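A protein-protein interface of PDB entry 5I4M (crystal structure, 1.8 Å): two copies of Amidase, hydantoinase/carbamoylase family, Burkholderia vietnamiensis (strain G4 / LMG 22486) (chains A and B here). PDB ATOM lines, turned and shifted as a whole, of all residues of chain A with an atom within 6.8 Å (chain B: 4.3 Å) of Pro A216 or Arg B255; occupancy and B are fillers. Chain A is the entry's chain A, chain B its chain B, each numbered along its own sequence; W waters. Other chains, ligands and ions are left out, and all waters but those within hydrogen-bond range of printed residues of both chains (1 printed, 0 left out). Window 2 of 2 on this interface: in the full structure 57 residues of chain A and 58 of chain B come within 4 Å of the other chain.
Water W1 bridges NH1 of Arg B255 and O of Asp A399.
The backbone NH (N) of Gln A214 sits at hydrogen-bond distance from the side-chain sulfur (SG) of Cys A397 (3.5 Å).
Of the 7 printed residues of chain B, 2 touch a printed residue of chain A.
Printed residues of chain B that touch a printed residue of chain A: Pro B250 and Arg B255.
Hydrophobic or aromatic side chains of chain B within 4 Å of the printed part of chain A: Pro B250.
Along chain B the printed residues that touch a printed residue of chain A span positions 250 to 255.
Of the 15 printed residues of chain A, 3 touch a printed residue of chain B.
Printed residues of chain A that touch a printed residue of chain B: Gln A214, Gly A215 and Pro A216.
Hydrophobic or aromatic side chains of chain A within 4 Å of the printed part of chain B: Pro A216.
Among the printed residues, 4 pairs touch across the chains.
No position is printed for both chains.
Of the 4 pairs that touch across the chains among the printed residues, none has its exchanged pair printed and touching as well.
Gln A214 touches Pro B250 (O to CG, 3.2 Å).
Gly A215 touches Pro B250.
O of Pro B250 touches CD of Pro A216 (3.97 Å).
Arg B255 touches Pro A216 (NH1 to CB, 3.6 Å).
Of chain B, only Pro B250 and Arg B255 come within 4 Å of Pro A216.
Of the printed residues of chain A, Pro B250 touches Gln A214, Gly A215 and Pro A216.
Of the printed residues of chain B, Gln A214 touches Pro B250.
Printed residues of chain B within 4 Å of Gly A215: Pro B250.
Glu A221 touches none of the printed residues of chain B.
The nearest residue of chain B that does not touch Pro A216 is Pro B252 (4.1 Å).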
ATOM      1  N   GLU A 213     -17.804 -18.788  -8.397  1.00  0.00           N
ATOM      2  CA  GLU A 213     -16.440 -19.262  -8.628  1.00  0.00           C
ATOM      3  C   GLU A 213     -16.397 -20.734  -9.044  1.00  0.00           C
ATOM      4  O   GLU A 213     -15.590 -21.120  -9.904  1.00  0.00           O
ATOM      5  CB  GLU A 213     -15.596 -19.059  -7.374  1.00  0.00           C
ATOM      6  CG  GLU A 213     -14.167 -19.561  -7.571  1.00  0.00           C
ATOM      7  CD  GLU A 213     -13.399 -19.659  -6.272  1.00  0.00           C
ATOM      8  OE1 GLU A 213     -12.457 -20.468  -6.200  1.00  0.00           O
ATOM      9  OE2 GLU A 213     -13.750 -18.943  -5.320  1.00  0.00           O
ATOM     10  N   GLN A 214     -17.224 -21.572  -8.412  1.00  0.00           N
ATOM     11  CA  GLN A 214     -17.236 -23.023  -8.579  1.00  0.00           C
ATOM     12  C   GLN A 214     -16.001 -23.683  -7.981  1.00  0.00           C
ATOM     13  O   GLN A 214     -15.711 -24.848  -8.277  1.00  0.00           O
ATOM     14  CB  GLN A 214     -17.398 -23.418 -10.052  1.00  0.00           C
ATOM     15  CG  GLN A 214     -18.654 -22.814 -10.663  1.00  0.00           C
ATOM     16  CD  GLN A 214     -18.804 -23.170 -12.118  1.00  0.00           C
ATOM     17  OE1 GLN A 214     -18.056 -22.676 -12.956  1.00  0.00           O
ATOM     18  NE2 GLN A 214     -19.778 -24.027 -12.430  1.00  0.00           N
ATOM     19  N   GLY A 215     -15.277 -22.951  -7.143  1.00  0.00           N
ATOM     20  CA  GLY A 215     -14.174 -23.477  -6.374  1.00  0.00           C
ATOM     21  C   GLY A 215     -14.099 -22.763  -5.037  1.00  0.00           C
ATOM     22  O   GLY A 215     -14.865 -21.830  -4.772  1.00  0.00           O
ATOM     23  N   PRO A 216     -13.151 -23.157  -4.187  1.00  0.00           N
ATOM     24  CA  PRO A 216     -13.189 -22.769  -2.770  1.00  0.00           C
ATOM     25  C   PRO A 216     -12.418 -21.512  -2.397  1.00  0.00           C
ATOM     26  O   PRO A 216     -12.449 -21.138  -1.219  1.00  0.00           O
ATOM     27  CB  PRO A 216     -12.550 -23.987  -2.100  1.00  0.00           C
ATOM     28  CG  PRO A 216     -11.473 -24.378  -3.090  1.00  0.00           C
ATOM     29  CD  PRO A 216     -12.134 -24.192  -4.450  1.00  0.00           C
ATOM     30  N   ILE A 217     -11.746 -20.861  -3.351  1.00  0.00           N
ATOM     31  CA  ILE A 217     -10.719 -19.868  -3.023  1.00  0.00           C
ATOM     32  C   ILE A 217     -11.331 -18.619  -2.408  1.00  0.00           C
ATOM     33  O   ILE A 217     -10.887 -18.152  -1.352  1.00  0.00           O
ATOM     34  CB  ILE A 217      -9.895 -19.523  -4.278  1.00  0.00           C
ATOM     35  CG1 ILE A 217      -9.097 -20.752  -4.731  1.00  0.00           C
ATOM     36  CG2 ILE A 217      -8.976 -18.339  -4.021  1.00  0.00           C
ATOM     37  CD1 ILE A 217      -8.445 -20.578  -6.097  1.00  0.00           C
ATOM     38  N   LEU A 218     -12.312 -18.016  -3.082  1.00  0.00           N
ATOM     39  CA  LEU A 218     -12.847 -16.755  -2.582  1.00  0.00           C
ATOM     40  C   LEU A 218     -13.448 -16.924  -1.193  1.00  0.00           C
ATOM     41  O   LEU A 218     -13.230 -16.086  -0.311  1.00  0.00           O
ATOM     42  CB  LEU A 218     -13.886 -16.192  -3.549  1.00  0.00           C
ATOM     43  CG  LEU A 218     -13.356 -15.798  -4.923  1.00  0.00           C
ATOM     44  CD1 LEU A 218     -14.518 -15.341  -5.826  1.00  0.00           C
ATOM     45  CD2 LEU A 218     -12.296 -14.700  -4.778  1.00  0.00           C
ATOM     46  N   GLU A 219     -14.205 -18.005  -0.975  1.00  0.00           N
ATOM     47  CA  GLU A 219     -14.752 -18.233   0.362  1.00  0.00           C
ATOM     48  C   GLU A 219     -13.643 -18.490   1.373  1.00  0.00           C
ATOM     49  O   GLU A 219     -13.676 -17.951   2.484  1.00  0.00           O
ATOM     50  CB  GLU A 219     -15.738 -19.404   0.361  1.00  0.00           C
ATOM     51  CG  GLU A 219     -16.255 -19.736   1.767  1.00  0.00           C
ATOM     52  CD  GLU A 219     -17.052 -21.028   1.812  1.00  0.00           C
ATOM     53  OE1 GLU A 219     -18.184 -21.008   2.333  1.00  0.00           O
ATOM     54  OE2 GLU A 219     -16.543 -22.065   1.328  1.00  0.00           O
ATOM     55  N   ALA A 220     -12.659 -19.318   1.012  1.00  0.00           N
ATOM     56  CA  ALA A 220     -11.613 -19.658   1.974  1.00  0.00           C
ATOM     57  C   ALA A 220     -10.764 -18.445   2.331  1.00  0.00           C
ATOM     58  O   ALA A 220     -10.220 -18.374   3.441  1.00  0.00           O
ATOM     59  CB  ALA A 220     -10.741 -20.791   1.430  1.00  0.00           C
ATOM     60  N   GLU A 221     -10.662 -17.473   1.430  1.00  0.00           N
ATOM     61  CA  GLU A 221      -9.802 -16.330   1.677  1.00  0.00           C
ATOM     62  C   GLU A 221     -10.584 -15.084   2.099  1.00  0.00           C
ATOM     63  O   GLU A 221     -10.016 -13.998   2.202  1.00  0.00           O
ATOM     64  CB  GLU A 221      -8.948 -16.053   0.438  1.00  0.00           C
ATOM     65  CG  GLU A 221      -8.022 -17.228   0.148  1.00  0.00           C
ATOM     66  CD  GLU A 221      -7.105 -17.019  -1.043  1.00  0.00           C
ATOM     67  OE1 GLU A 221      -6.418 -17.993  -1.421  1.00  0.00           O
ATOM     68  OE2 GLU A 221      -7.068 -15.900  -1.589  1.00  0.00           O
ATOM     69  N   PRO A 396     -18.086 -15.936  -4.415  1.00  0.00           N
ATOM     70  CA  PRO A 396     -17.765 -17.259  -3.860  1.00  0.00           C
ATOM     71  C   PRO A 396     -18.949 -18.201  -3.977  1.00  0.00           C
ATOM     72  O   PRO A 396     -20.059 -17.806  -4.328  1.00  0.00           O
ATOM     73  CB  PRO A 396     -17.441 -16.978  -2.384  1.00  0.00           C
ATOM     74  CG  PRO A 396     -17.308 -15.485  -2.266  1.00  0.00           C
ATOM     75  CD  PRO A 396     -18.161 -14.911  -3.358  1.00  0.00           C
ATOM     76  N   CYS A 397     -18.700 -19.472  -3.662  1.00  0.00           N
ATOM     77  CA  CYS A 397     -19.787 -20.407  -3.410  1.00  0.00           C
ATOM     78  C   CYS A 397     -19.424 -21.276  -2.215  1.00  0.00           C
ATOM     79  O   CYS A 397     -18.246 -21.474  -1.910  1.00  0.00           O
ATOM     80  CB  CYS A 397     -20.120 -21.280  -4.629  1.00  0.00           C
ATOM     81  SG  CYS A 397     -18.720 -22.170  -5.333  1.00  0.00           S
ATOM     82  N   ILE A 398     -20.458 -21.780  -1.537  1.00  0.00           N
ATOM     83  CA  ILE A 398     -20.278 -22.439  -0.247  1.00  0.00           C
ATOM     84  C   ILE A 398     -19.475 -23.717  -0.432  1.00  0.00           C
ATOM     85  O   ILE A 398     -19.832 -24.585  -1.243  1.00  0.00           O
ATOM     86  CB  ILE A 398     -21.638 -22.736   0.404  1.00  0.00           C
ATOM     87  CG1 ILE A 398     -22.350 -21.442   0.780  1.00  0.00           C
ATOM     88  CG2 ILE A 398     -21.457 -23.634   1.616  1.00  0.00           C
ATOM     89  CD1 ILE A 398     -21.730 -20.718   1.955  1.00  0.00           C
ATOM     90  N   ASP A 399     -18.378 -23.836   0.325  1.00  0.00           N
ATOM     91  CA  ASP A 399     -17.486 -24.991   0.284  1.00  0.00           C
ATOM     92  C   ASP A 399     -16.900 -25.203  -1.107  1.00  0.00           C
ATOM     93  O   ASP A 399     -16.332 -26.265  -1.399  1.00  0.00           O
ATOM     94  CB  ASP A 399     -18.198 -26.260   0.777  1.00  0.00           C
ATOM     95  CG  ASP A 399     -18.667 -26.137   2.224  1.00  0.00           C
ATOM     96  OD1 ASP A 399     -17.968 -25.483   3.023  1.00  0.00           O
ATOM     97  OD2 ASP A 399     -19.744 -26.673   2.558  1.00  0.00           O
ATOM     98  N   GLY A 400     -17.020 -24.185  -1.957  1.00  0.00           N
ATOM     99  CA  GLY A 400     -16.531 -24.218  -3.318  1.00  0.00           C
ATOM    100  C   GLY A 400     -17.130 -25.277  -4.211  1.00  0.00           C
ATOM    101  O   GLY A 400     -16.535 -25.606  -5.238  1.00  0.00           O
ATOM    102  N   ILE A 401     -18.308 -25.811  -3.889  1.00  0.00           N
ATOM    103  CA  ILE A 401     -18.833 -26.934  -4.655  1.00  0.00           C
ATOM    104  C   ILE A 401     -19.772 -26.431  -5.742  1.00  0.00           C
ATOM    105  O   ILE A 401     -20.576 -25.509  -5.542  1.00  0.00           O
ATOM    106  CB  ILE A 401     -19.518 -27.976  -3.751  1.00  0.00           C
ATOM    107  CG1 ILE A 401     -19.908 -29.199  -4.596  1.00  0.00           C
ATOM    108  CG2 ILE A 401     -20.712 -27.383  -3.049  1.00  0.00           C
ATOM    109  CD1 ILE A 401     -19.526 -30.534  -3.981  1.00  0.00           C
ATOM    110  N   PRO B 250     -12.750 -26.849 -11.393  1.00  0.00           N
ATOM    111  CA  PRO B 250     -12.171 -26.211 -10.201  1.00  0.00           C
ATOM    112  C   PRO B 250     -12.393 -26.924  -8.871  1.00  0.00           C
ATOM    113  O   PRO B 250     -12.250 -26.287  -7.825  1.00  0.00           O
ATOM    114  CB  PRO B 250     -12.835 -24.823 -10.190  1.00  0.00           C
ATOM    115  CG  PRO B 250     -14.067 -24.968 -11.022  1.00  0.00           C
ATOM    116  CD  PRO B 250     -13.759 -25.997 -12.051  1.00  0.00           C
ATOM    117  N   PRO B 252     -10.481 -28.978  -6.432  1.00  0.00           N
ATOM    118  CA  PRO B 252      -9.056 -29.334  -6.321  1.00  0.00           C
ATOM    119  C   PRO B 252      -8.868 -30.842  -6.262  1.00  0.00           C
ATOM    120  O   PRO B 252      -9.580 -31.541  -5.542  1.00  0.00           O
ATOM    121  CB  PRO B 252      -8.620 -28.653  -5.018  1.00  0.00           C
ATOM    122  CG  PRO B 252      -9.572 -27.502  -4.866  1.00  0.00           C
ATOM    123  CD  PRO B 252     -10.890 -28.023  -5.384  1.00  0.00           C
ATOM    124  N   MET B 253      -7.917 -31.339  -7.055  1.00  0.00           N
ATOM    125  CA  MET B 253      -7.719 -32.783  -7.184  1.00  0.00           C
ATOM    126  C   MET B 253      -7.566 -33.506  -5.855  1.00  0.00           C
ATOM    127  O   MET B 253      -8.135 -34.602  -5.719  1.00  0.00           O
ATOM    128  CB  MET B 253      -6.488 -33.094  -8.054  1.00  0.00           C
ATOM    129  CG  MET B 253      -6.608 -32.748  -9.535  1.00  0.00           C
ATOM    130  SD  MET B 253      -7.824 -33.736 -10.405  1.00  0.00           S
ATOM    131  CE  MET B 253      -7.055 -35.362 -10.421  1.00  0.00           C
ATOM    132  N   PRO B 254      -6.824 -32.996  -4.867  1.00  0.00           N
ATOM    133  CA  PRO B 254      -6.600 -33.799  -3.656  1.00  0.00           C
ATOM    134  C   PRO B 254      -7.836 -33.985  -2.796  1.00  0.00           C
ATOM    135  O   PRO B 254      -7.867 -34.931  -2.001  1.00  0.00           O
ATOM    136  CB  PRO B 254      -5.514 -33.014  -2.909  1.00  0.00           C
ATOM    137  CG  PRO B 254      -4.843 -32.218  -3.958  1.00  0.00           C
ATOM    138  CD  PRO B 254      -5.948 -31.810  -4.876  1.00  0.00           C
ATOM    139  N   ARG B 255      -8.851 -33.132  -2.914  1.00  0.00           N
ATOM    140  CA  ARG B 255     -10.028 -33.251  -2.060  1.00  0.00           C
ATOM    141  C   ARG B 255     -11.194 -33.955  -2.748  1.00  0.00           C
ATOM    142  O   ARG B 255     -12.290 -34.021  -2.183  1.00  0.00           O
ATOM    143  CB  ARG B 255     -10.472 -31.873  -1.564  1.00  0.00           C
ATOM    144  CG  ARG B 255     -11.165 -31.022  -2.618  1.00  0.00           C
ATOM    145  CD  ARG B 255     -11.784 -29.760  -2.006  1.00  0.00           C
ATOM    146  NE  ARG B 255     -10.773 -28.835  -1.492  1.00  0.00           N
ATOM    147  CZ  ARG B 255     -11.054 -27.665  -0.920  1.00  0.00           C
ATOM    148  NH1 ARG B 255     -12.320 -27.280  -0.786  1.00  0.00           N
ATOM    149  NH2 ARG B 255     -10.072 -26.880  -0.483  1.00  0.00           N
ATOM    150  N   ARG B 256     -10.989 -34.490  -3.943  1.00  0.00           N
ATOM    151  CA  ARG B 256     -12.075 -35.149  -4.650  1.00  0.00           C
ATOM    152  C   ARG B 256     -12.383 -36.512  -4.039  1.00  0.00           C
ATOM    153  O   ARG B 256     -11.502 -37.201  -3.523  1.00  0.00           O
ATOM    154  CB  ARG B 256     -11.718 -35.328  -6.118  1.00  0.00           C
ATOM    155  CG  ARG B 256     -11.444 -34.024  -6.815  1.00  0.00           C
ATOM    156  CD  ARG B 256     -11.033 -34.271  -8.232  1.00  0.00           C
ATOM    157  NE  ARG B 256     -10.924 -33.015  -8.955  1.00  0.00           N
ATOM    158  CZ  ARG B 256     -11.102 -32.910 -10.265  1.00  0.00           C
ATOM    159  NH1 ARG B 256     -11.379 -33.994 -10.983  1.00  0.00           N
ATOM    160  NH2 ARG B 256     -10.992 -31.726 -10.853  1.00  0.00           N
ATOM    161  N   ARG B 257     -13.656 -36.895  -4.109  1.00  0.00           N
ATOM    162  CA  ARG B 257     -14.128 -38.218  -3.703  1.00  0.00           C
ATOM    163  C   ARG B 257     -14.844 -38.818  -4.909  1.00  0.00           C
ATOM    164  O   ARG B 257     -16.070 -38.787  -5.014  1.00  0.00           O
ATOM    165  CB  ARG B 257     -15.028 -38.123  -2.451  1.00  0.00           C
ATOM    166  CG  ARG B 257     -14.292 -37.500  -1.268  1.00  0.00           C
ATOM    167  CD  ARG B 257     -14.986 -37.755   0.067  1.00  0.00           C
ATOM    168  NE  ARG B 257     -16.312 -37.155   0.147  1.00  0.00           N
ATOM    169  CZ  ARG B 257     -17.439 -37.842   0.336  1.00  0.00           C
ATOM    170  NH1 ARG B 257     -17.416 -39.165   0.469  1.00  0.00           N
ATOM    171  NH2 ARG B 257     -18.596 -37.200   0.403  1.00  0.00           N
HETATM  172  O   HOH W   1     -14.218 -27.839  -3.391  1.00  0.00           O
